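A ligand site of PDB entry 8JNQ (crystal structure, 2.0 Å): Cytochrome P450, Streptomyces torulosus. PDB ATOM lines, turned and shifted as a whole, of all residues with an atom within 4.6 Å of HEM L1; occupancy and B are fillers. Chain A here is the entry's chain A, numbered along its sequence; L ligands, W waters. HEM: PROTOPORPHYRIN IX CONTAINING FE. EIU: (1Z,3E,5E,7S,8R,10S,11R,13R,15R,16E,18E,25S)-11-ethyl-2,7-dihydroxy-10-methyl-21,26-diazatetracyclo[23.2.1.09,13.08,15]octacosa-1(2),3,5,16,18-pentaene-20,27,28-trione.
SG of Cys 345 binds FE of HEM L1 (2.3 Å). An oxygen (O2D) of HEM L1 sits at hydrogen-bond distance from a ring nitrogen (NE2) of His 91, at 2.5 Å. A ring nitrogen (ND1) of His 343 lies within hydrogen-bond range of an oxygen (O1D) of HEM L1 (2.6 Å). NH2 of Arg 287 is in salt-bridge range of O2A of HEM L1 (2.7 Å). An oxygen (O2D) of HEM L1 is in salt-bridge range of the guanidinium group of Arg 95 (3.1 Å).
The backbone NH (N) of Gly 347 lies close to the side-chain sulfur (SG) of Cys 345, at 3.1 Å. ND1 of His 343 sits at hydrogen-bond distance from NE2 of His 91. ND1 of His 343 lies close to O of Leu 83 (3.2 Å). The guanidinium group (NH1) of Arg 287 lies within hydrogen-bond range of the backbone carbonyl oxygen (O) of Leu 285, 3.1 Å away. The guanidinium group (NH1) of Arg 95 is in hydrogen-bond range of the backbone carbonyl oxygen (O) of Val 342, 3.4 Å away. O of Tyr 344 is in hydrogen-bond range of NH1 of Arg 95 (2.7 Å). OG1 of Thr 238 is in hydrogen-bond range of OG of Ser 237, 3.5 Å away. The side-chain amide nitrogen (NE2) of Gln 241 is in hydrogen-bond range of the side-chain sulfur (SD) of Met 274 (3.6 Å).
The backbone carbonyl oxygen (O) of Leu 83 sits close to an oxygen (O1D) of HEM L1. CZ of Phe 84 touches CAD of HEM L1 (3.2 Å). CE1 of Phe 102 touches CBC of HEM L1, at 3.6 Å. Ile 147 touches HEM L1. Leu 230 touches HEM L1. Ala 233 touches HEM L1. N of Gly 234 touches CAC of HEM L1, at 3.95 Å. OG of Ser 237 touches CHC of HEM L1, 3.2 Å away. Thr 238 touches HEM L1 (OG1 to CAB, 3.8 Å). Gln 241 touches HEM L1 (CG to CBB, 3.8 Å). Met 274 touches HEM L1 (CE to CMB, 3.8 Å). Leu 279 touches HEM L1 (CD2 to CMB, 3.4 Å). O of Gly 337 touches CMB of HEM L1, at 3.6 Å. C of Phe 338 touches CMA of HEM L1 (3.7 Å). Gly 339 touches HEM L1. Val 342 touches HEM L1 (O to O2D, 3.8 Å). Val 346 touches HEM L1 (CG1 to CMD, 3.5 Å). CA of Gly 347 touches C3C of HEM L1 (3.7 Å). Ala 351 touches HEM L1 (CB to CAB, 3.8 Å). Hydrophobic or aromatic side chains that line HEM L1: Leu 83, Phe 84, His 91, Phe 102, Ile 147, Leu 230, Ala 233, Met 274, Leu 279, Phe 338, His 343, Val 346 and Ala 351. Within 4 Å of HEM L1: Leu 83, Phe 84, His 91, Arg 95, Phe 102, Ile 147, Leu 230, Ala 233, Gly 234, Ser 237, Thr 238, Gln 241, Met 274, Leu 279, Arg 287, Gly 337, Phe 338, Gly 339, Val 342, His 343, Cys 345, Val 346, Gly 347 and Ala 351. The nearest printed residue that does not touch HEM L1 is Leu 280 (4.1 Å).
Water W2 lies within hydrogen-bond range of O1A of HEM L1 (2.6 Å), O36 of EIU L2 (2.9 Å) and N of Leu 285 (2.9 Å).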
ATOM      1  N   LEU A  55      28.272 -20.590 -15.192  1.00  0.00           N
ATOM      2  CA  LEU A  55      27.090 -21.347 -14.783  1.00  0.00           C
ATOM      3  C   LEU A  55      26.681 -22.389 -15.822  1.00  0.00           C
ATOM      4  O   LEU A  55      26.046 -23.390 -15.467  1.00  0.00           O
ATOM      5  CB  LEU A  55      25.933 -20.390 -14.493  1.00  0.00           C
ATOM      6  CG  LEU A  55      26.118 -19.544 -13.229  1.00  0.00           C
ATOM      7  CD1 LEU A  55      24.923 -18.561 -13.007  1.00  0.00           C
ATOM      8  CD2 LEU A  55      26.298 -20.474 -12.054  1.00  0.00           C
ATOM      9  N   LEU A  83      22.146 -31.986  -4.445  1.00  0.00           N
ATOM     10  CA  LEU A  83      22.027 -31.075  -5.580  1.00  0.00           C
ATOM     11  C   LEU A  83      23.204 -30.120  -5.678  1.00  0.00           C
ATOM     12  O   LEU A  83      23.661 -29.785  -6.777  1.00  0.00           O
ATOM     13  CB  LEU A  83      20.711 -30.300  -5.488  1.00  0.00           C
ATOM     14  CG  LEU A  83      19.473 -31.191  -5.618  1.00  0.00           C
ATOM     15  CD1 LEU A  83      18.218 -30.437  -5.282  1.00  0.00           C
ATOM     16  CD2 LEU A  83      19.411 -31.790  -7.034  1.00  0.00           C
ATOM     17  N   PHE A  84      23.690 -29.625  -4.540  1.00  0.00           N
ATOM     18  CA  PHE A  84      24.816 -28.687  -4.552  1.00  0.00           C
ATOM     19  C   PHE A  84      26.166 -29.389  -4.661  1.00  0.00           C
ATOM     20  O   PHE A  84      27.197 -28.712  -4.627  1.00  0.00           O
ATOM     21  CB  PHE A  84      24.772 -27.816  -3.295  1.00  0.00           C
ATOM     22  CG  PHE A  84      23.566 -26.916  -3.213  1.00  0.00           C
ATOM     23  CD1 PHE A  84      23.467 -25.798  -4.022  1.00  0.00           C
ATOM     24  CD2 PHE A  84      22.537 -27.174  -2.326  1.00  0.00           C
ATOM     25  CE1 PHE A  84      22.371 -24.944  -3.928  1.00  0.00           C
ATOM     26  CE2 PHE A  84      21.437 -26.321  -2.246  1.00  0.00           C
ATOM     27  CZ  PHE A  84      21.351 -25.221  -3.048  1.00  0.00           C
ATOM     28  N   HIS A  91      23.407 -35.422 -10.957  1.00  0.00           N
ATOM     29  CA  HIS A  91      22.554 -34.313 -10.546  1.00  0.00           C
ATOM     30  C   HIS A  91      21.172 -34.436 -11.175  1.00  0.00           C
ATOM     31  O   HIS A  91      20.139 -34.251 -10.505  1.00  0.00           O
ATOM     32  CB  HIS A  91      23.210 -32.981 -10.913  1.00  0.00           C
ATOM     33  CG  HIS A  91      22.330 -31.777 -10.676  1.00  0.00           C
ATOM     34  ND1 HIS A  91      21.340 -31.395 -11.554  1.00  0.00           N
ATOM     35  CD2 HIS A  91      22.297 -30.880  -9.657  1.00  0.00           C
ATOM     36  CE1 HIS A  91      20.723 -30.314 -11.086  1.00  0.00           C
ATOM     37  NE2 HIS A  91      21.298 -29.981  -9.931  1.00  0.00           N
ATOM     38  N   ARG A  95      17.530 -34.185  -9.384  1.00  0.00           N
ATOM     39  CA  ARG A  95      16.678 -33.034  -9.677  1.00  0.00           C
ATOM     40  C   ARG A  95      15.380 -33.458 -10.373  1.00  0.00           C
ATOM     41  O   ARG A  95      14.330 -32.837 -10.149  1.00  0.00           O
ATOM     42  CB  ARG A  95      17.486 -32.030 -10.492  1.00  0.00           C
ATOM     43  CG  ARG A  95      16.699 -30.892 -11.139  1.00  0.00           C
ATOM     44  CD  ARG A  95      16.596 -29.708 -10.209  1.00  0.00           C
ATOM     45  NE  ARG A  95      15.970 -28.572 -10.867  1.00  0.00           N
ATOM     46  CZ  ARG A  95      16.505 -27.359 -10.946  1.00  0.00           C
ATOM     47  NH1 ARG A  95      17.682 -27.083 -10.410  1.00  0.00           N
ATOM     48  NH2 ARG A  95      15.824 -26.396 -11.556  1.00  0.00           N
ATOM     49  N   PHE A 102       7.926 -28.816  -7.860  1.00  0.00           N
ATOM     50  CA  PHE A 102       8.298 -27.406  -7.873  1.00  0.00           C
ATOM     51  C   PHE A 102       8.034 -26.736  -9.215  1.00  0.00           C
ATOM     52  O   PHE A 102       8.336 -25.551  -9.351  1.00  0.00           O
ATOM     53  CB  PHE A 102       9.772 -27.245  -7.478  1.00  0.00           C
ATOM     54  CG  PHE A 102      10.011 -27.413  -5.999  1.00  0.00           C
ATOM     55  CD1 PHE A 102       9.788 -26.370  -5.120  1.00  0.00           C
ATOM     56  CD2 PHE A 102      10.445 -28.626  -5.495  1.00  0.00           C
ATOM     57  CE1 PHE A 102      10.010 -26.515  -3.771  1.00  0.00           C
ATOM     58  CE2 PHE A 102      10.667 -28.788  -4.144  1.00  0.00           C
ATOM     59  CZ  PHE A 102      10.452 -27.722  -3.270  1.00  0.00           C
ATOM     60  N   ILE A 147       6.774 -23.684   2.871  1.00  0.00           N
ATOM     61  CA  ILE A 147       7.676 -24.788   2.558  1.00  0.00           C
ATOM     62  C   ILE A 147       7.388 -25.988   3.465  1.00  0.00           C
ATOM     63  O   ILE A 147       7.430 -27.140   3.031  1.00  0.00           O
ATOM     64  CB  ILE A 147       9.154 -24.364   2.641  1.00  0.00           C
ATOM     65  CG1 ILE A 147      10.037 -25.418   1.955  1.00  0.00           C
ATOM     66  CG2 ILE A 147       9.629 -24.195   4.093  1.00  0.00           C
ATOM     67  CD1 ILE A 147       9.592 -25.754   0.518  1.00  0.00           C
ATOM     68  N   LEU A 230      16.169 -28.743   0.549  1.00  0.00           N
ATOM     69  CA  LEU A 230      14.931 -28.023   0.275  1.00  0.00           C
ATOM     70  C   LEU A 230      14.458 -27.279   1.514  1.00  0.00           C
ATOM     71  O   LEU A 230      14.033 -26.115   1.437  1.00  0.00           O
ATOM     72  CB  LEU A 230      13.870 -28.996  -0.245  1.00  0.00           C
ATOM     73  CG  LEU A 230      14.155 -29.661  -1.601  1.00  0.00           C
ATOM     74  CD1 LEU A 230      13.115 -30.716  -1.904  1.00  0.00           C
ATOM     75  CD2 LEU A 230      14.215 -28.621  -2.723  1.00  0.00           C
ATOM     76  N   ALA A 233      16.976 -24.260   2.144  1.00  0.00           N
ATOM     77  CA  ALA A 233      16.729 -23.266   1.098  1.00  0.00           C
ATOM     78  C   ALA A 233      15.405 -22.548   1.330  1.00  0.00           C
ATOM     79  O   ALA A 233      15.326 -21.313   1.281  1.00  0.00           O
ATOM     80  CB  ALA A 233      16.741 -23.943  -0.287  1.00  0.00           C
ATOM     81  N   GLY A 234      14.331 -23.316   1.572  1.00  0.00           N
ATOM     82  CA  GLY A 234      13.041 -22.686   1.801  1.00  0.00           C
ATOM     83  C   GLY A 234      13.037 -21.772   3.001  1.00  0.00           C
ATOM     84  O   GLY A 234      12.256 -20.814   3.053  1.00  0.00           O
ATOM     85  N   SER A 237      15.859 -18.160   2.268  1.00  0.00           N
ATOM     86  CA  SER A 237      15.875 -17.353   1.054  1.00  0.00           C
ATOM     87  C   SER A 237      14.763 -16.312   1.061  1.00  0.00           C
ATOM     88  O   SER A 237      15.008 -15.118   1.300  1.00  0.00           O
ATOM     89  CB  SER A 237      15.780 -18.275  -0.161  1.00  0.00           C
ATOM     90  OG  SER A 237      14.596 -19.081  -0.124  1.00  0.00           O
ATOM     91  N   THR A 238      13.534 -16.753   0.812  1.00  0.00           N
ATOM     92  CA  THR A 238      12.406 -15.832   0.657  1.00  0.00           C
ATOM     93  C   THR A 238      12.150 -15.027   1.930  1.00  0.00           C
ATOM     94  O   THR A 238      11.712 -13.881   1.850  1.00  0.00           O
ATOM     95  CB  THR A 238      11.167 -16.619   0.252  1.00  0.00           C
ATOM     96  OG1 THR A 238      11.522 -17.581  -0.745  1.00  0.00           O
ATOM     97  CG2 THR A 238      10.175 -15.704  -0.382  1.00  0.00           C
ATOM     98  N   GLN A 241      14.235 -12.118   1.383  1.00  0.00           N
ATOM     99  CA  GLN A 241      13.900 -11.386   0.157  1.00  0.00           C
ATOM    100  C   GLN A 241      12.575 -10.642   0.276  1.00  0.00           C
ATOM    101  O   GLN A 241      12.420  -9.556  -0.291  1.00  0.00           O
ATOM    102  CB  GLN A 241      13.853 -12.335  -1.042  1.00  0.00           C
ATOM    103  CG  GLN A 241      13.896 -11.620  -2.418  1.00  0.00           C
ATOM    104  CD  GLN A 241      15.288 -11.037  -2.724  1.00  0.00           C
ATOM    105  OE1 GLN A 241      15.885 -10.363  -1.894  1.00  0.00           O
ATOM    106  NE2 GLN A 241      15.794 -11.300  -3.930  1.00  0.00           N
ATOM    107  N   MET A 274      14.179  -8.791  -8.208  1.00  0.00           N
ATOM    108  CA  MET A 274      15.116  -9.916  -8.242  1.00  0.00           C
ATOM    109  C   MET A 274      16.455  -9.495  -8.843  1.00  0.00           C
ATOM    110  O   MET A 274      17.527  -9.844  -8.328  1.00  0.00           O
ATOM    111  CB  MET A 274      14.515 -11.071  -9.052  1.00  0.00           C
ATOM    112  CG  MET A 274      13.522 -11.986  -8.320  1.00  0.00           C
ATOM    113  SD  MET A 274      14.148 -12.763  -6.798  1.00  0.00           S
ATOM    114  CE  MET A 274      15.434 -13.766  -7.604  1.00  0.00           C
ATOM    115  N   LEU A 279      21.683  -9.895  -2.776  1.00  0.00           N
ATOM    116  CA  LEU A 279      21.166 -10.798  -1.751  1.00  0.00           C
ATOM    117  C   LEU A 279      22.233 -11.688  -1.143  1.00  0.00           C
ATOM    118  O   LEU A 279      22.269 -11.855   0.072  1.00  0.00           O
ATOM    119  CB  LEU A 279      20.063 -11.680  -2.333  1.00  0.00           C
ATOM    120  CG  LEU A 279      19.370 -12.701  -1.416  1.00  0.00           C
ATOM    121  CD1 LEU A 279      18.356 -11.994  -0.497  1.00  0.00           C
ATOM    122  CD2 LEU A 279      18.687 -13.749  -2.260  1.00  0.00           C
ATOM    123  N   LEU A 280      23.097 -12.275  -1.959  1.00  0.00           N
ATOM    124  CA  LEU A 280      23.927 -13.417  -1.553  1.00  0.00           C
ATOM    125  C   LEU A 280      25.297 -12.899  -1.154  1.00  0.00           C
ATOM    126  O   LEU A 280      26.213 -12.811  -1.974  1.00  0.00           O
ATOM    127  CB  LEU A 280      24.043 -14.428  -2.676  1.00  0.00           C
ATOM    128  CG  LEU A 280      22.732 -15.024  -3.135  1.00  0.00           C
ATOM    129  CD1 LEU A 280      22.929 -15.868  -4.406  1.00  0.00           C
ATOM    130  CD2 LEU A 280      22.143 -15.866  -2.009  1.00  0.00           C
ATOM    131  N   LEU A 285      28.506 -20.677  -3.932  1.00  0.00           N
ATOM    132  CA  LEU A 285      29.324 -21.882  -4.046  1.00  0.00           C
ATOM    133  C   LEU A 285      30.363 -21.734  -5.154  1.00  0.00           C
ATOM    134  O   LEU A 285      30.019 -21.451  -6.306  1.00  0.00           O
ATOM    135  CB  LEU A 285      28.458 -23.109  -4.319  1.00  0.00           C
ATOM    136  CG  LEU A 285      27.481 -23.377  -3.187  1.00  0.00           C
ATOM    137  CD1 LEU A 285      26.586 -24.556  -3.533  1.00  0.00           C
ATOM    138  CD2 LEU A 285      28.260 -23.641  -1.953  1.00  0.00           C
ATOM    139  N   ARG A 287      32.800 -22.999  -7.969  1.00  0.00           N
ATOM    140  CA  ARG A 287      33.032 -24.130  -8.846  1.00  0.00           C
ATOM    141  C   ARG A 287      34.525 -24.351  -9.010  1.00  0.00           C
ATOM    142  O   ARG A 287      35.329 -23.418  -8.948  1.00  0.00           O
ATOM    143  CB  ARG A 287      32.384 -23.854 -10.203  1.00  0.00           C
ATOM    144  CG  ARG A 287      30.915 -24.178 -10.236  1.00  0.00           C
ATOM    145  CD  ARG A 287      30.074 -23.026  -9.818  1.00  0.00           C
ATOM    146  NE  ARG A 287      28.680 -23.262 -10.154  1.00  0.00           N
ATOM    147  CZ  ARG A 287      27.642 -22.834  -9.449  1.00  0.00           C
ATOM    148  NH1 ARG A 287      27.811 -22.125  -8.346  1.00  0.00           N
ATOM    149  NH2 ARG A 287      26.413 -23.120  -9.849  1.00  0.00           N
ATOM    150  N   GLY A 337      19.259 -13.655 -11.023  1.00  0.00           N
ATOM    151  CA  GLY A 337      18.906 -13.694  -9.613  1.00  0.00           C
ATOM    152  C   GLY A 337      18.523 -15.073  -9.100  1.00  0.00           C
ATOM    153  O   GLY A 337      18.561 -15.298  -7.885  1.00  0.00           O
ATOM    154  N   PHE A 338      18.092 -15.977  -9.978  1.00  0.00           N
ATOM    155  CA  PHE A 338      17.838 -17.378  -9.627  1.00  0.00           C
ATOM    156  C   PHE A 338      18.905 -18.317 -10.185  1.00  0.00           C
ATOM    157  O   PHE A 338      18.678 -19.527 -10.228  1.00  0.00           O
ATOM    158  CB  PHE A 338      16.457 -17.835 -10.134  1.00  0.00           C
ATOM    159  CG  PHE A 338      15.295 -17.312  -9.335  1.00  0.00           C
ATOM    160  CD1 PHE A 338      15.138 -17.635  -7.994  1.00  0.00           C
ATOM    161  CD2 PHE A 338      14.321 -16.521  -9.942  1.00  0.00           C
ATOM    162  CE1 PHE A 338      14.048 -17.131  -7.252  1.00  0.00           C
ATOM    163  CE2 PHE A 338      13.241 -16.019  -9.209  1.00  0.00           C
ATOM    164  CZ  PHE A 338      13.103 -16.330  -7.859  1.00  0.00           C
ATOM    165  N   GLY A 339      20.052 -17.797 -10.621  1.00  0.00           N
ATOM    166  CA  GLY A 339      21.058 -18.665 -11.226  1.00  0.00           C
ATOM    167  C   GLY A 339      20.809 -18.955 -12.694  1.00  0.00           C
ATOM    168  O   GLY A 339      20.060 -18.260 -13.387  1.00  0.00           O
ATOM    169  N   VAL A 342      22.522 -25.964 -14.862  1.00  0.00           N
ATOM    170  CA  VAL A 342      21.860 -27.107 -14.249  1.00  0.00           C
ATOM    171  C   VAL A 342      21.414 -26.798 -12.821  1.00  0.00           C
ATOM    172  O   VAL A 342      20.400 -27.323 -12.361  1.00  0.00           O
ATOM    173  CB  VAL A 342      22.769 -28.361 -14.296  1.00  0.00           C
ATOM    174  CG1 VAL A 342      23.522 -28.472 -15.660  1.00  0.00           C
ATOM    175  CG2 VAL A 342      23.700 -28.393 -13.145  1.00  0.00           C
ATOM    176  N   HIS A 343      22.131 -25.930 -12.106  1.00  0.00           N
ATOM    177  CA  HIS A 343      21.746 -25.606 -10.730  1.00  0.00           C
ATOM    178  C   HIS A 343      20.764 -24.443 -10.634  1.00  0.00           C
ATOM    179  O   HIS A 343      20.536 -23.951  -9.522  1.00  0.00           O
ATOM    180  CB  HIS A 343      22.998 -25.316  -9.905  1.00  0.00           C
ATOM    181  CG  HIS A 343      23.949 -26.467  -9.865  1.00  0.00           C
ATOM    182  ND1 HIS A 343      23.711 -27.598  -9.094  1.00  0.00           N
ATOM    183  CD2 HIS A 343      25.094 -26.713 -10.551  1.00  0.00           C
ATOM    184  CE1 HIS A 343      24.697 -28.458  -9.281  1.00  0.00           C
ATOM    185  NE2 HIS A 343      25.537 -27.952 -10.162  1.00  0.00           N
ATOM    186  N   TYR A 344      20.176 -24.010 -11.762  1.00  0.00           N
ATOM    187  CA  TYR A 344      19.134 -22.990 -11.737  1.00  0.00           C
ATOM    188  C   TYR A 344      18.109 -23.290 -10.634  1.00  0.00           C
ATOM    189  O   TYR A 344      17.660 -24.420 -10.489  1.00  0.00           O
ATOM    190  CB  TYR A 344      18.430 -22.914 -13.108  1.00  0.00           C
ATOM    191  CG  TYR A 344      17.290 -21.916 -13.169  1.00  0.00           C
ATOM    192  CD1 TYR A 344      17.534 -20.565 -13.416  1.00  0.00           C
ATOM    193  CD2 TYR A 344      15.982 -22.305 -12.935  1.00  0.00           C
ATOM    194  CE1 TYR A 344      16.506 -19.628 -13.449  1.00  0.00           C
ATOM    195  CE2 TYR A 344      14.948 -21.380 -12.972  1.00  0.00           C
ATOM    196  CZ  TYR A 344      15.221 -20.052 -13.215  1.00  0.00           C
ATOM    197  OH  TYR A 344      14.198 -19.146 -13.259  1.00  0.00           O
ATOM    198  N   CYS A 345      17.716 -22.258  -9.893  1.00  0.00           N
ATOM    199  CA  CYS A 345      16.976 -22.495  -8.647  1.00  0.00           C
ATOM    200  C   CYS A 345      15.764 -23.402  -8.853  1.00  0.00           C
ATOM    201  O   CYS A 345      14.859 -23.075  -9.618  1.00  0.00           O
ATOM    202  CB  CYS A 345      16.539 -21.166  -8.052  1.00  0.00           C
ATOM    203  SG  CYS A 345      15.447 -21.310  -6.606  1.00  0.00           S
ATOM    204  N   VAL A 346      15.718 -24.531  -8.144  1.00  0.00           N
ATOM    205  CA  VAL A 346      14.543 -25.381  -8.263  1.00  0.00           C
ATOM    206  C   VAL A 346      13.343 -24.763  -7.542  1.00  0.00           C
ATOM    207  O   VAL A 346      12.187 -25.138  -7.815  1.00  0.00           O
ATOM    208  CB  VAL A 346      14.839 -26.798  -7.726  1.00  0.00           C
ATOM    209  CG1 VAL A 346      14.848 -26.789  -6.200  1.00  0.00           C
ATOM    210  CG2 VAL A 346      13.791 -27.771  -8.242  1.00  0.00           C
ATOM    211  N   GLY A 347      13.574 -23.815  -6.650  1.00  0.00           N
ATOM    212  CA  GLY A 347      12.482 -23.142  -5.987  1.00  0.00           C
ATOM    213  C   GLY A 347      11.998 -21.884  -6.684  1.00  0.00           C
ATOM    214  O   GLY A 347      11.221 -21.134  -6.082  1.00  0.00           O
ATOM    215  N   LEU A 350       8.120 -21.330  -6.892  1.00  0.00           N
ATOM    216  CA  LEU A 350       7.560 -21.132  -5.557  1.00  0.00           C
ATOM    217  C   LEU A 350       7.946 -19.777  -4.976  1.00  0.00           C
ATOM    218  O   LEU A 350       7.091 -19.045  -4.471  1.00  0.00           O
ATOM    219  CB  LEU A 350       7.999 -22.259  -4.628  1.00  0.00           C
ATOM    220  CG  LEU A 350       7.492 -22.171  -3.195  1.00  0.00           C
ATOM    221  CD1 LEU A 350       6.009 -22.428  -3.168  1.00  0.00           C
ATOM    222  CD2 LEU A 350       8.216 -23.167  -2.306  1.00  0.00           C
ATOM    223  N   ALA A 351       9.243 -19.432  -5.012  1.00  0.00           N
ATOM    224  CA  ALA A 351       9.666 -18.113  -4.514  1.00  0.00           C
ATOM    225  C   ALA A 351       8.939 -16.992  -5.252  1.00  0.00           C
ATOM    226  O   ALA A 351       8.421 -16.051  -4.640  1.00  0.00           O
ATOM    227  CB  ALA A 351      11.168 -17.961  -4.677  1.00  0.00           C
ATOM    228  N   LEU A 355       6.671 -14.155  -3.447  1.00  0.00           N
ATOM    229  CA  LEU A 355       6.982 -12.726  -3.500  1.00  0.00           C
ATOM    230  C   LEU A 355       5.826 -11.947  -4.119  1.00  0.00           C
ATOM    231  O   LEU A 355       5.463 -10.866  -3.631  1.00  0.00           O
ATOM    232  CB  LEU A 355       8.277 -12.503  -4.285  1.00  0.00           C
ATOM    233  CG  LEU A 355       9.533 -13.163  -3.688  1.00  0.00           C
ATOM    234  CD1 LEU A 355      10.649 -13.238  -4.710  1.00  0.00           C
ATOM    235  CD2 LEU A 355      10.003 -12.424  -2.462  1.00  0.00           C
HETATM  236  CHA HEM L   1      19.667 -22.855  -6.202  1.00  0.00           C
HETATM  237  CHB HEM L   1      18.397 -18.218  -5.485  1.00  0.00           C
HETATM  238  CHC HEM L   1      14.350 -19.643  -3.218  1.00  0.00           C
HETATM  239  CHD HEM L   1      15.966 -24.213  -3.410  1.00  0.00           C
HETATM  240  C1A HEM L   1      19.646 -21.479  -6.237  1.00  0.00           C
HETATM  241  C2A HEM L   1      20.623 -20.636  -6.891  1.00  0.00           C
HETATM  242  C3A HEM L   1      20.269 -19.367  -6.699  1.00  0.00           C
HETATM  243  C4A HEM L   1      19.062 -19.352  -5.912  1.00  0.00           C
HETATM  244  CMA HEM L   1      21.012 -18.113  -7.204  1.00  0.00           C
HETATM  245  CAA HEM L   1      21.866 -21.130  -7.688  1.00  0.00           C
HETATM  246  CBA HEM L   1      23.063 -21.305  -6.764  1.00  0.00           C
HETATM  247  CGA HEM L   1      24.291 -21.698  -7.549  1.00  0.00           C
HETATM  248  O1A HEM L   1      25.369 -21.771  -6.925  1.00  0.00           O
HETATM  249  O2A HEM L   1      24.195 -21.947  -8.785  1.00  0.00           O
HETATM  250  C1B HEM L   1      17.221 -18.199  -4.793  1.00  0.00           C
HETATM  251  C2B HEM L   1      16.505 -17.013  -4.376  1.00  0.00           C
HETATM  252  C3B HEM L   1      15.386 -17.390  -3.725  1.00  0.00           C
HETATM  253  C4B HEM L   1      15.344 -18.841  -3.739  1.00  0.00           C
HETATM  254  CMB HEM L   1      17.032 -15.599  -4.654  1.00  0.00           C
HETATM  255  CAB HEM L   1      14.274 -16.525  -3.112  1.00  0.00           C
HETATM  256  CBB HEM L   1      14.141 -15.246  -3.454  1.00  0.00           C
HETATM  257  C1C HEM L   1      14.420 -21.021  -3.104  1.00  0.00           C
HETATM  258  C2C HEM L   1      13.434 -21.869  -2.492  1.00  0.00           C
HETATM  259  C3C HEM L   1      13.891 -23.138  -2.545  1.00  0.00           C
HETATM  260  C4C HEM L   1      15.173 -23.113  -3.200  1.00  0.00           C
HETATM  261  CMC HEM L   1      12.105 -21.320  -1.909  1.00  0.00           C
HETATM  262  CAC HEM L   1      13.276 -24.477  -2.055  1.00  0.00           C
HETATM  263  CBC HEM L   1      12.038 -24.531  -1.573  1.00  0.00           C
HETATM  264  C1D HEM L   1      17.107 -24.231  -4.176  1.00  0.00           C
HETATM  265  C2D HEM L   1      17.877 -25.423  -4.464  1.00  0.00           C
HETATM  266  C3D HEM L   1      18.910 -25.062  -5.234  1.00  0.00           C
HETATM  267  C4D HEM L   1      18.807 -23.628  -5.457  1.00  0.00           C
HETATM  268  CMD HEM L   1      17.524 -26.834  -3.924  1.00  0.00           C
HETATM  269  CAD HEM L   1      19.989 -26.009  -5.808  1.00  0.00           C
HETATM  270  CBD HEM L   1      19.483 -26.499  -7.175  1.00  0.00           C
HETATM  271  CGD HEM L   1      20.449 -27.435  -7.858  1.00  0.00           C
HETATM  272  O1D HEM L   1      21.672 -27.391  -7.571  1.00  0.00           O
HETATM  273  O2D HEM L   1      19.974 -28.216  -8.729  1.00  0.00           O
HETATM  274  NA  HEM L   1      18.693 -20.660  -5.652  1.00  0.00           N
HETATM  275  NB  HEM L   1      16.484 -19.303  -4.388  1.00  0.00           N
HETATM  276  NC  HEM L   1      15.463 -21.815  -3.537  1.00  0.00           N
HETATM  277  ND  HEM L   1      17.704 -23.158  -4.788  1.00  0.00           N
HETATM  278 FE   HEM L   1      16.916 -21.259  -4.835  1.00  0.00          FE
HETATM  279  C1  EIU L   2      21.728 -22.995   0.174  1.00  0.00           C
HETATM  280  C10 EIU L   2      19.468 -17.671  -0.719  1.00  0.00           C
HETATM  281  C11 EIU L   2      22.013 -19.397  -3.001  1.00  0.00           C
HETATM  282  C12 EIU L   2      23.723 -22.489  -1.382  1.00  0.00           C
HETATM  283  C13 EIU L   2      24.773 -22.705  -0.297  1.00  0.00           C
HETATM  284  C14 EIU L   2      25.052 -23.911   0.246  1.00  0.00           C
HETATM  285  C15 EIU L   2      22.422 -23.196   1.520  1.00  0.00           C
HETATM  286  C16 EIU L   2      22.578 -24.563   2.116  1.00  0.00           C
HETATM  287  C17 EIU L   2      26.116 -24.067   1.305  1.00  0.00           C
HETATM  288  C18 EIU L   2      26.292 -25.131   2.076  1.00  0.00           C
HETATM  289  C19 EIU L   2      23.186 -24.617   3.300  1.00  0.00           C
HETATM  290  C2  EIU L   2      22.423 -21.972  -0.728  1.00  0.00           C
HETATM  291  C20 EIU L   2      23.124 -25.656   4.161  1.00  0.00           C
HETATM  292  C21 EIU L   2      27.318 -25.286   3.092  1.00  0.00           C
HETATM  293  C24 EIU L   2      25.927 -28.655   6.161  1.00  0.00           C
HETATM  294  C25 EIU L   2      24.493 -26.973   7.390  1.00  0.00           C
HETATM  295  C26 EIU L   2      25.897 -27.518   7.192  1.00  0.00           C
HETATM  296  C27 EIU L   2      28.398 -26.486   5.019  1.00  0.00           C
HETATM  297  C28 EIU L   2      27.388 -26.355   3.959  1.00  0.00           C
HETATM  298  C3  EIU L   2      20.319 -22.410   0.361  1.00  0.00           C
HETATM  299  C30 EIU L   2      27.027 -28.416   5.131  1.00  0.00           C
HETATM  300  C31 EIU L   2      26.566 -27.548   3.956  1.00  0.00           C
HETATM  301  C34 EIU L   2      23.935 -25.608   5.421  1.00  0.00           C
HETATM  302  C4  EIU L   2      19.963 -21.997  -1.082  1.00  0.00           C
HETATM  303  C5  EIU L   2      21.297 -21.502  -1.699  1.00  0.00           C
HETATM  304  C6  EIU L   2      18.977 -20.819  -1.133  1.00  0.00           C
HETATM  305  C7  EIU L   2      19.663 -19.845  -2.093  1.00  0.00           C
HETATM  306  C8  EIU L   2      21.175 -19.972  -1.851  1.00  0.00           C
HETATM  307  C9  EIU L   2      19.169 -18.388  -2.034  1.00  0.00           C
HETATM  308  N23 EIU L   2      23.803 -26.744   6.120  1.00  0.00           N
HETATM  309  N29 EIU L   2      28.158 -27.660   5.643  1.00  0.00           N
HETATM  310  O22 EIU L   2      28.256 -24.331   3.153  1.00  0.00           O
HETATM  311  O32 EIU L   2      29.284 -25.689   5.300  1.00  0.00           O
HETATM  312  O33 EIU L   2      25.678 -27.874   3.185  1.00  0.00           O
HETATM  313  O35 EIU L   2      24.646 -24.672   5.808  1.00  0.00           O
HETATM  314  O36 EIU L   2      24.202 -21.468  -2.261  1.00  0.00           O
HETATM  315  O   HOH W   1      22.715 -21.499 -11.005  1.00  0.00           O
HETATM  316  O   HOH W   2      25.692 -20.733  -4.587  1.00  0.00           O
